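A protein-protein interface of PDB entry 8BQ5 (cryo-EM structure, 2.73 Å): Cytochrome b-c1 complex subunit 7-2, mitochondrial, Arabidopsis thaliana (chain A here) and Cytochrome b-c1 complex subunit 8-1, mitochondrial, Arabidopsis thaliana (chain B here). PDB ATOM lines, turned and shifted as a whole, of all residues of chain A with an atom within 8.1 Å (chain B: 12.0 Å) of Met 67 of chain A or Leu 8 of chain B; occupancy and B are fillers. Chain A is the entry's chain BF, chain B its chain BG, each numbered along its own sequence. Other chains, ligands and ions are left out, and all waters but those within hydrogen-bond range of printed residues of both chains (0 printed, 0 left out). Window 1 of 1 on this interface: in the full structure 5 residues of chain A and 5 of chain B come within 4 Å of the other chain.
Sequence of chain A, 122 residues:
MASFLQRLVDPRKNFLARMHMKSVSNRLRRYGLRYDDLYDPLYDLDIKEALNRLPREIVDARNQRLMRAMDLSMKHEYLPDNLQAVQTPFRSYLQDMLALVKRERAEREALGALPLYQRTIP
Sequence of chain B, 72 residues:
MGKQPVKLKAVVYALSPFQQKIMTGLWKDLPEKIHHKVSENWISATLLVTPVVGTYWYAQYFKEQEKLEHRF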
ATOM      1  N   TYR A  31     -12.935 -12.247  14.158  1.00  0.00           N
ATOM      2  CA  TYR A  31     -12.148 -12.678  13.013  1.00  0.00           C
ATOM      3  C   TYR A  31     -11.237 -11.589  12.468  1.00  0.00           C
ATOM      4  O   TYR A  31     -10.477 -11.852  11.530  1.00  0.00           O
ATOM      5  CB  TYR A  31     -13.074 -13.175  11.898  1.00  0.00           C
ATOM      6  CG  TYR A  31     -13.693 -14.522  12.173  1.00  0.00           C
ATOM      7  CD1 TYR A  31     -12.928 -15.679  12.137  1.00  0.00           C
ATOM      8  CD2 TYR A  31     -15.045 -14.640  12.467  1.00  0.00           C
ATOM      9  CE1 TYR A  31     -13.490 -16.914  12.386  1.00  0.00           C
ATOM     10  CE2 TYR A  31     -15.615 -15.868  12.718  1.00  0.00           C
ATOM     11  CZ  TYR A  31     -14.833 -17.002  12.676  1.00  0.00           C
ATOM     12  OH  TYR A  31     -15.397 -18.230  12.925  1.00  0.00           O
ATOM     13  N   LEU A  33     -12.336  -8.968  10.889  1.00  0.00           N
ATOM     14  CA  LEU A  33     -12.946  -8.615   9.618  1.00  0.00           C
ATOM     15  C   LEU A  33     -13.681  -7.288   9.727  1.00  0.00           C
ATOM     16  O   LEU A  33     -14.283  -6.980  10.759  1.00  0.00           O
ATOM     17  CB  LEU A  33     -13.928  -9.697   9.169  1.00  0.00           C
ATOM     18  CG  LEU A  33     -13.365 -10.961   8.528  1.00  0.00           C
ATOM     19  CD1 LEU A  33     -14.480 -11.970   8.319  1.00  0.00           C
ATOM     20  CD2 LEU A  33     -12.677 -10.634   7.214  1.00  0.00           C
ATOM     21  N   ASP A  37     -15.504  -6.264   4.127  1.00  0.00           N
ATOM     22  CA  ASP A  37     -14.777  -7.470   3.653  1.00  0.00           C
ATOM     23  C   ASP A  37     -15.776  -8.579   3.300  1.00  0.00           C
ATOM     24  O   ASP A  37     -15.379  -9.499   2.569  1.00  0.00           O
ATOM     25  CB  ASP A  37     -13.777  -7.984   4.686  1.00  0.00           C
ATOM     26  CG  ASP A  37     -12.748  -6.987   5.184  1.00  0.00           C
ATOM     27  OD1 ASP A  37     -12.501  -5.997   4.491  1.00  0.00           O
ATOM     28  OD2 ASP A  37     -12.189  -7.229   6.263  1.00  0.00           O
ATOM     29  N   ARG A  56      -4.315   0.350  -4.286  1.00  0.00           N
ATOM     30  CA  ARG A  56      -3.763  -0.984  -4.077  1.00  0.00           C
ATOM     31  C   ARG A  56      -3.570  -1.291  -2.597  1.00  0.00           C
ATOM     32  O   ARG A  56      -3.752  -2.434  -2.165  1.00  0.00           O
ATOM     33  CB  ARG A  56      -2.438  -1.119  -4.827  1.00  0.00           C
ATOM     34  CG  ARG A  56      -2.050  -2.548  -5.157  1.00  0.00           C
ATOM     35  CD  ARG A  56      -0.550  -2.758  -5.032  1.00  0.00           C
ATOM     36  NE  ARG A  56      -0.190  -4.167  -5.134  1.00  0.00           N
ATOM     37  CZ  ARG A  56       0.989  -4.668  -4.792  1.00  0.00           C
ATOM     38  NH1 ARG A  56       1.956  -3.900  -4.316  1.00  0.00           N
ATOM     39  NH2 ARG A  56       1.203  -5.974  -4.930  1.00  0.00           N
ATOM     40  N   VAL A  59      -6.820  -2.561  -1.072  1.00  0.00           N
ATOM     41  CA  VAL A  59      -7.201  -3.891  -1.540  1.00  0.00           C
ATOM     42  C   VAL A  59      -6.246  -4.947  -0.993  1.00  0.00           C
ATOM     43  O   VAL A  59      -6.661  -6.064  -0.665  1.00  0.00           O
ATOM     44  CB  VAL A  59      -7.266  -3.918  -3.077  1.00  0.00           C
ATOM     45  CG1 VAL A  59      -7.750  -5.274  -3.563  1.00  0.00           C
ATOM     46  CG2 VAL A  59      -8.183  -2.819  -3.582  1.00  0.00           C
ATOM     47  N   ASP A  60      -4.956  -4.618  -0.896  1.00  0.00           N
ATOM     48  CA  ASP A  60      -4.005  -5.554  -0.306  1.00  0.00           C
ATOM     49  C   ASP A  60      -4.331  -5.818   1.159  1.00  0.00           C
ATOM     50  O   ASP A  60      -4.229  -6.957   1.629  1.00  0.00           O
ATOM     51  CB  ASP A  60      -2.579  -5.022  -0.452  1.00  0.00           C
ATOM     52  CG  ASP A  60      -2.027  -5.205  -1.853  1.00  0.00           C
ATOM     53  OD1 ASP A  60      -2.647  -5.941  -2.650  1.00  0.00           O
ATOM     54  OD2 ASP A  60      -0.969  -4.614  -2.157  1.00  0.00           O
ATOM     55  N   ALA A  61      -4.714  -4.774   1.897  1.00  0.00           N
ATOM     56  CA  ALA A  61      -5.076  -4.950   3.300  1.00  0.00           C
ATOM     57  C   ALA A  61      -6.360  -5.756   3.446  1.00  0.00           C
ATOM     58  O   ALA A  61      -6.492  -6.564   4.373  1.00  0.00           O
ATOM     59  CB  ALA A  61      -5.215  -3.589   3.982  1.00  0.00           C
ATOM     60  N   ARG A  62      -7.325  -5.523   2.554  1.00  0.00           N
ATOM     61  CA  ARG A  62      -8.582  -6.318   2.563  1.00  0.00           C
ATOM     62  C   ARG A  62      -8.230  -7.790   2.347  1.00  0.00           C
ATOM     63  O   ARG A  62      -8.735  -8.625   3.110  1.00  0.00           O
ATOM     64  CB  ARG A  62      -9.554  -5.823   1.491  1.00  0.00           C
ATOM     65  CG  ARG A  62     -10.630  -6.825   1.102  1.00  0.00           C
ATOM     66  CD  ARG A  62     -11.260  -6.525  -0.242  1.00  0.00           C
ATOM     67  NE  ARG A  62     -12.120  -7.620  -0.665  1.00  0.00           N
ATOM     68  CZ  ARG A  62     -13.436  -7.671  -0.496  1.00  0.00           C
ATOM     69  NH1 ARG A  62     -14.078  -6.674   0.088  1.00  0.00           N
ATOM     70  NH2 ARG A  62     -14.109  -8.725  -0.919  1.00  0.00           N
ATOM     71  N   ASN A  63      -7.382  -8.093   1.363  1.00  0.00           N
ATOM     72  CA  ASN A  63      -7.039  -9.504   1.036  1.00  0.00           C
ATOM     73  C   ASN A  63      -6.330 -10.170   2.219  1.00  0.00           C
ATOM     74  O   ASN A  63      -6.510 -11.382   2.392  1.00  0.00           O
ATOM     75  CB  ASN A  63      -6.203  -9.600  -0.243  1.00  0.00           C
ATOM     76  CG  ASN A  63      -6.957  -9.185  -1.489  1.00  0.00           C
ATOM     77  OD1 ASN A  63      -8.171  -9.348  -1.570  1.00  0.00           O
ATOM     78  ND2 ASN A  63      -6.244  -8.655  -2.466  1.00  0.00           N
ATOM     79  N   GLN A  64      -5.552  -9.415   2.993  1.00  0.00           N
ATOM     80  CA  GLN A  64      -4.779 -10.004   4.119  1.00  0.00           C
ATOM     81  C   GLN A  64      -5.722 -10.276   5.293  1.00  0.00           C
ATOM     82  O   GLN A  64      -5.542 -11.304   5.952  1.00  0.00           O
ATOM     83  CB  GLN A  64      -3.617  -9.088   4.499  1.00  0.00           C
ATOM     84  CG  GLN A  64      -2.478  -9.106   3.491  1.00  0.00           C
ATOM     85  CD  GLN A  64      -1.439  -8.050   3.773  1.00  0.00           C
ATOM     86  OE1 GLN A  64      -1.515  -7.322   4.759  1.00  0.00           O
ATOM     87  NE2 GLN A  64      -0.453  -7.957   2.897  1.00  0.00           N
ATOM     88  N   ARG A  65      -6.687  -9.387   5.538  1.00  0.00           N
ATOM     89  CA  ARG A  65      -7.699  -9.622   6.601  1.00  0.00           C
ATOM     90  C   ARG A  65      -8.519 -10.856   6.238  1.00  0.00           C
ATOM     91  O   ARG A  65      -8.826 -11.632   7.147  1.00  0.00           O
ATOM     92  CB  ARG A  65      -8.637  -8.424   6.729  1.00  0.00           C
ATOM     93  CG  ARG A  65      -8.065  -7.253   7.508  1.00  0.00           C
ATOM     94  CD  ARG A  65      -9.114  -6.188   7.737  1.00  0.00           C
ATOM     95  NE  ARG A  65      -9.677  -5.610   6.525  1.00  0.00           N
ATOM     96  CZ  ARG A  65      -9.244  -4.507   5.929  1.00  0.00           C
ATOM     97  NH1 ARG A  65      -8.207  -3.845   6.411  1.00  0.00           N
ATOM     98  NH2 ARG A  65      -9.846  -4.069   4.842  1.00  0.00           N
ATOM     99  N   LEU A  66      -8.828 -11.030   4.952  1.00  0.00           N
ATOM    100  CA  LEU A  66      -9.619 -12.198   4.488  1.00  0.00           C
ATOM    101  C   LEU A  66      -8.811 -13.489   4.672  1.00  0.00           C
ATOM    102  O   LEU A  66      -9.410 -14.479   5.098  1.00  0.00           O
ATOM    103  CB  LEU A  66     -10.013 -11.986   3.024  1.00  0.00           C
ATOM    104  CG  LEU A  66     -11.131 -10.977   2.773  1.00  0.00           C
ATOM    105  CD1 LEU A  66     -11.361 -10.791   1.283  1.00  0.00           C
ATOM    106  CD2 LEU A  66     -12.414 -11.414   3.453  1.00  0.00           C
ATOM    107  N   MET A  67      -7.507 -13.467   4.380  1.00  0.00           N
ATOM    108  CA  MET A  67      -6.653 -14.673   4.549  1.00  0.00           C
ATOM    109  C   MET A  67      -6.497 -14.982   6.040  1.00  0.00           C
ATOM    110  O   MET A  67      -6.507 -16.171   6.384  1.00  0.00           O
ATOM    111  CB  MET A  67      -5.263 -14.507   3.930  1.00  0.00           C
ATOM    112  CG  MET A  67      -4.590 -15.843   3.685  1.00  0.00           C
ATOM    113  SD  MET A  67      -2.862 -15.734   3.184  1.00  0.00           S
ATOM    114  CE  MET A  67      -2.466 -17.472   3.009  1.00  0.00           C
ATOM    115  N   ARG A  68      -6.338 -13.956   6.878  1.00  0.00           N
ATOM    116  CA  ARG A  68      -6.263 -14.165   8.346  1.00  0.00           C
ATOM    117  C   ARG A  68      -7.572 -14.795   8.831  1.00  0.00           C
ATOM    118  O   ARG A  68      -7.497 -15.775   9.575  1.00  0.00           O
ATOM    119  CB  ARG A  68      -5.982 -12.830   9.041  1.00  0.00           C
ATOM    120  CG  ARG A  68      -6.041 -12.859  10.560  1.00  0.00           C
ATOM    121  CD  ARG A  68      -5.599 -11.530  11.143  1.00  0.00           C
ATOM    122  NE  ARG A  68      -6.494 -10.430  10.810  1.00  0.00           N
ATOM    123  CZ  ARG A  68      -6.426  -9.217  11.345  1.00  0.00           C
ATOM    124  NH1 ARG A  68      -5.500  -8.938  12.246  1.00  0.00           N
ATOM    125  NH2 ARG A  68      -7.284  -8.282  10.978  1.00  0.00           N
ATOM    126  N   ALA A  69      -8.717 -14.264   8.401  1.00  0.00           N
ATOM    127  CA  ALA A  69     -10.031 -14.771   8.854  1.00  0.00           C
ATOM    128  C   ALA A  69     -10.252 -16.211   8.390  1.00  0.00           C
ATOM    129  O   ALA A  69     -10.769 -16.994   9.192  1.00  0.00           O
ATOM    130  CB  ALA A  69     -11.120 -13.883   8.334  1.00  0.00           C
ATOM    131  N   MET A  70      -9.896 -16.530   7.140  1.00  0.00           N
ATOM    132  CA  MET A  70     -10.089 -17.902   6.602  1.00  0.00           C
ATOM    133  C   MET A  70      -9.140 -18.852   7.329  1.00  0.00           C
ATOM    134  O   MET A  70      -9.523 -20.009   7.521  1.00  0.00           O
ATOM    135  CB  MET A  70      -9.832 -17.961   5.094  1.00  0.00           C
ATOM    136  CG  MET A  70     -10.840 -17.176   4.281  1.00  0.00           C
ATOM    137  SD  MET A  70     -11.947 -18.208   3.299  1.00  0.00           S
ATOM    138  CE  MET A  70     -10.782 -19.377   2.605  1.00  0.00           C
ATOM    139  N   ASP A  71      -7.957 -18.375   7.715  1.00  0.00           N
ATOM    140  CA  ASP A  71      -7.002 -19.191   8.505  1.00  0.00           C
ATOM    141  C   ASP A  71      -7.591 -19.433   9.898  1.00  0.00           C
ATOM    142  O   ASP A  71      -7.576 -20.588  10.330  1.00  0.00           O
ATOM    143  CB  ASP A  71      -5.637 -18.507   8.552  1.00  0.00           C
ATOM    144  CG  ASP A  71      -4.617 -19.186   9.444  1.00  0.00           C
ATOM    145  OD1 ASP A  71      -4.195 -20.302   9.100  1.00  0.00           O
ATOM    146  OD2 ASP A  71      -4.244 -18.583  10.469  1.00  0.00           O
ATOM    147  N   LEU A  72      -8.119 -18.392  10.555  1.00  0.00           N
ATOM    148  CA  LEU A  72      -8.740 -18.578  11.862  1.00  0.00           C
ATOM    149  C   LEU A  72      -9.930 -19.524  11.780  1.00  0.00           C
ATOM    150  O   LEU A  72     -10.102 -20.394  12.642  1.00  0.00           O
ATOM    151  CB  LEU A  72      -9.175 -17.230  12.437  1.00  0.00           C
ATOM    152  CG  LEU A  72      -8.077 -16.276  12.902  1.00  0.00           C
ATOM    153  CD1 LEU A  72      -8.661 -14.899  13.161  1.00  0.00           C
ATOM    154  CD2 LEU A  72      -7.392 -16.812  14.143  1.00  0.00           C
ATOM    155  N   SER A  73     -10.769 -19.364  10.754  1.00  0.00           N
ATOM    156  CA  SER A  73     -11.948 -20.213  10.618  1.00  0.00           C
ATOM    157  C   SER A  73     -11.556 -21.666  10.381  1.00  0.00           C
ATOM    158  O   SER A  73     -12.201 -22.584  10.901  1.00  0.00           O
ATOM    159  CB  SER A  73     -12.833 -19.697   9.484  1.00  0.00           C
ATOM    160  OG  SER A  73     -13.730 -20.698   9.038  1.00  0.00           O
ATOM    161  N   MET A  74     -10.503 -21.892   9.593  1.00  0.00           N
ATOM    162  CA  MET A  74     -10.019 -23.250   9.367  1.00  0.00           C
ATOM    163  C   MET A  74      -9.479 -23.875  10.646  1.00  0.00           C
ATOM    164  O   MET A  74      -9.682 -25.069  10.888  1.00  0.00           O
ATOM    165  CB  MET A  74      -8.945 -23.247   8.278  1.00  0.00           C
ATOM    166  CG  MET A  74      -8.305 -24.603   8.022  1.00  0.00           C
ATOM    167  SD  MET A  74      -6.679 -24.786   8.778  1.00  0.00           S
ATOM    168  CE  MET A  74      -5.774 -23.468   7.973  1.00  0.00           C
ATOM    169  N   PRO B   5      -5.322 -14.279 -10.724  1.00  0.00           N
ATOM    170  CA  PRO B   5      -4.504 -14.515  -9.529  1.00  0.00           C
ATOM    171  C   PRO B   5      -4.412 -13.285  -8.630  1.00  0.00           C
ATOM    172  O   PRO B   5      -4.181 -12.178  -9.117  1.00  0.00           O
ATOM    173  CB  PRO B   5      -3.131 -14.873 -10.107  1.00  0.00           C
ATOM    174  CG  PRO B   5      -3.114 -14.264 -11.463  1.00  0.00           C
ATOM    175  CD  PRO B   5      -4.525 -14.311 -11.962  1.00  0.00           C
ATOM    176  N   VAL B   6      -4.580 -13.515  -7.322  1.00  0.00           N
ATOM    177  CA  VAL B   6      -4.548 -12.405  -6.326  1.00  0.00           C
ATOM    178  C   VAL B   6      -3.111 -12.204  -5.845  1.00  0.00           C
ATOM    179  O   VAL B   6      -2.480 -13.189  -5.422  1.00  0.00           O
ATOM    180  CB  VAL B   6      -5.511 -12.684  -5.153  1.00  0.00           C
ATOM    181  CG1 VAL B   6      -5.459 -14.130  -4.685  1.00  0.00           C
ATOM    182  CG2 VAL B   6      -5.307 -11.728  -3.988  1.00  0.00           C
ATOM    183  N   LYS B   7      -2.636 -10.955  -5.888  1.00  0.00           N
ATOM    184  CA  LYS B   7      -1.279 -10.632  -5.373  1.00  0.00           C
ATOM    185  C   LYS B   7      -1.303 -10.744  -3.847  1.00  0.00           C
ATOM    186  O   LYS B   7      -2.207 -10.153  -3.229  1.00  0.00           O
ATOM    187  CB  LYS B   7      -0.831  -9.248  -5.853  1.00  0.00           C
ATOM    188  CG  LYS B   7      -0.331  -9.194  -7.290  1.00  0.00           C
ATOM    189  CD  LYS B   7       0.348  -7.886  -7.625  1.00  0.00           C
ATOM    190  CE  LYS B   7       1.174  -7.950  -8.891  1.00  0.00           C
ATOM    191  NZ  LYS B   7       2.014  -6.740  -9.052  1.00  0.00           N
ATOM    192  N   LEU B   8      -0.343 -11.465  -3.268  1.00  0.00           N
ATOM    193  CA  LEU B   8      -0.361 -11.710  -1.804  1.00  0.00           C
ATOM    194  C   LEU B   8       1.033 -11.526  -1.205  1.00  0.00           C
ATOM    195  O   LEU B   8       2.007 -11.974  -1.837  1.00  0.00           O
ATOM    196  CB  LEU B   8      -0.857 -13.143  -1.589  1.00  0.00           C
ATOM    197  CG  LEU B   8      -1.126 -13.550  -0.143  1.00  0.00           C
ATOM    198  CD1 LEU B   8      -2.215 -12.683   0.469  1.00  0.00           C
ATOM    199  CD2 LEU B   8      -1.512 -15.019  -0.076  1.00  0.00           C
ATOM    200  N   LYS B   9       1.121 -10.880  -0.040  1.00  0.00           N
ATOM    201  CA  LYS B   9       2.416 -10.742   0.677  1.00  0.00           C
ATOM    202  C   LYS B   9       2.261 -11.445   2.028  1.00  0.00           C
ATOM    203  O   LYS B   9       1.467 -10.951   2.849  1.00  0.00           O
ATOM    204  CB  LYS B   9       2.784  -9.263   0.819  1.00  0.00           C
ATOM    205  CG  LYS B   9       4.047  -8.963   1.615  1.00  0.00           C
ATOM    206  CD  LYS B   9       5.324  -9.439   0.959  1.00  0.00           C
ATOM    207  CE  LYS B   9       6.561  -8.966   1.691  1.00  0.00           C
ATOM    208  NZ  LYS B   9       7.803  -9.517   1.104  1.00  0.00           N
ATOM    209  N   ALA B  10       2.981 -12.550   2.248  1.00  0.00           N
ATOM    210  CA  ALA B  10       2.795 -13.334   3.490  1.00  0.00           C
ATOM    211  C   ALA B  10       3.982 -14.250   3.784  1.00  0.00           C
ATOM    212  O   ALA B  10       4.698 -14.606   2.843  1.00  0.00           O
ATOM    213  CB  ALA B  10       1.541 -14.155   3.372  1.00  0.00           C
ATOM    214  N   VAL B  11       4.188 -14.601   5.051  1.00  0.00           N
ATOM    215  CA  VAL B  11       5.207 -15.563   5.452  1.00  0.00           C
ATOM    216  C   VAL B  11       4.514 -16.673   6.229  1.00  0.00           C
ATOM    217  O   VAL B  11       3.795 -16.401   7.197  1.00  0.00           O
ATOM    218  CB  VAL B  11       6.317 -14.910   6.295  1.00  0.00           C
ATOM    219  CG1 VAL B  11       7.303 -15.959   6.765  1.00  0.00           C
ATOM    220  CG2 VAL B  11       7.032 -13.837   5.494  1.00  0.00           C
ATOM    221  N   VAL B  12       4.724 -17.915   5.803  1.00  0.00           N
ATOM    222  CA  VAL B  12       4.047 -19.072   6.377  1.00  0.00           C
ATOM    223  C   VAL B  12       5.099 -20.058   6.863  1.00  0.00           C
ATOM    224  O   VAL B  12       5.980 -20.463   6.095  1.00  0.00           O
ATOM    225  CB  VAL B  12       3.102 -19.741   5.366  1.00  0.00           C
ATOM    226  CG1 VAL B  12       2.263 -20.803   6.051  1.00  0.00           C
ATOM    227  CG2 VAL B  12       2.212 -18.704   4.703  1.00  0.00           C
ATOM    228  N   TYR B  13       5.004 -20.443   8.131  1.00  0.00           N
ATOM    229  CA  TYR B  13       5.842 -21.485   8.708  1.00  0.00           C
ATOM    230  C   TYR B  13       4.987 -22.715   8.968  1.00  0.00           C
ATOM    231  O   TYR B  13       3.913 -22.611   9.567  1.00  0.00           O
ATOM    232  CB  TYR B  13       6.497 -21.022  10.009  1.00  0.00           C
ATOM    233  CG  TYR B  13       7.138 -19.656   9.949  1.00  0.00           C
ATOM    234  CD1 TYR B  13       6.386 -18.504  10.133  1.00  0.00           C
ATOM    235  CD2 TYR B  13       8.500 -19.520   9.725  1.00  0.00           C
ATOM    236  CE1 TYR B  13       6.970 -17.257  10.084  1.00  0.00           C
ATOM    237  CE2 TYR B  13       9.093 -18.278   9.675  1.00  0.00           C
ATOM    238  CZ  TYR B  13       8.324 -17.150   9.856  1.00  0.00           C
ATOM    239  OH  TYR B  13       8.911 -15.909   9.806  1.00  0.00           O
ATOM    240  N   ALA B  14       5.461 -23.873   8.521  1.00  0.00           N
ATOM    241  CA  ALA B  14       4.729 -25.119   8.682  1.00  0.00           C
ATOM    242  C   ALA B  14       5.650 -26.196   9.232  1.00  0.00           C
ATOM    243  O   ALA B  14       6.857 -26.194   8.982  1.00  0.00           O
ATOM    244  CB  ALA B  14       4.108 -25.582   7.362  1.00  0.00           C
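NE of Arg 56 of chain A is in salt-bridge range of OD2 of Asp 60 of chain A.
The side-chain amide nitrogen (ND2) of Asn 63 of chain A sits at hydrogen-bond distance from the backbone carbonyl oxygen (O) of Val 59 of chain A.
CD of Lys 7 of chain B touches NH2 of Arg 56 of chain A, 3.4 Å away.
Val 6 of chain B touches Asn 63 of chain A (CG2 to ND2, 3.6 Å).
NE2 of Gln 64 of chain A touches O of Lys 9 of chain B, 3.6 Å away.
Leu 8 of chain B touches Met 67 of chain A.
Met 67 of chain A touches one residue of chain B.
Of chain B, only Val 6 comes within 4 Å of Asn 63 of chain A.
Gln 64 of chain A touches one residue of chain B.
No residue of chain B comes within 4 Å of Leu 66 of chain A.
Ala 69 of chain A touches none of the printed residues of chain B.
Met 70 of chain A touches none of the printed residues of chain B.
No residue of chain B comes within 4 Å of Asp 71 of chain A.
Printed residues of chain A within 4 Å of Lys 9 of chain B: Gln 64 (3.6 Å).
Printed residues of chain A within 4 Å of Lys 7 of chain B: Arg 56.
Printed residues of chain A within 4 Å of Val 6 of chain B: Asn 63 (3.6 Å).
Of the printed residues of chain B, Arg 56 of chain A touches Lys 7 (3.4 Å).
Arg 68 of chain A touches none of the printed residues of chain B.
Ala 61 of chain A touches none of the printed residues of chain B.
The nearest residue of chain B that does not touch Met 67 of chain A is Ala 10 of chain B (4.7 Å).
The nearest residue of chain A that does not touch Leu 8 of chain B is Gln 64 of chain A (4.7 Å).
The nearest printed residue of chain A that does not touch Lys 9 of chain B is Met 67 of chain A (6.5 Å).
Of the 20 printed residues of chain A, 4 touch a printed residue of chain B.
Printed residues of chain A that touch a printed residue of chain B: Arg 56, Asn 63, Gln 64 and Met 67.
Of the 10 printed residues of chain B, 4 touch a printed residue of chain A.
Among the printed residues, 4 pairs touch across the chains.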
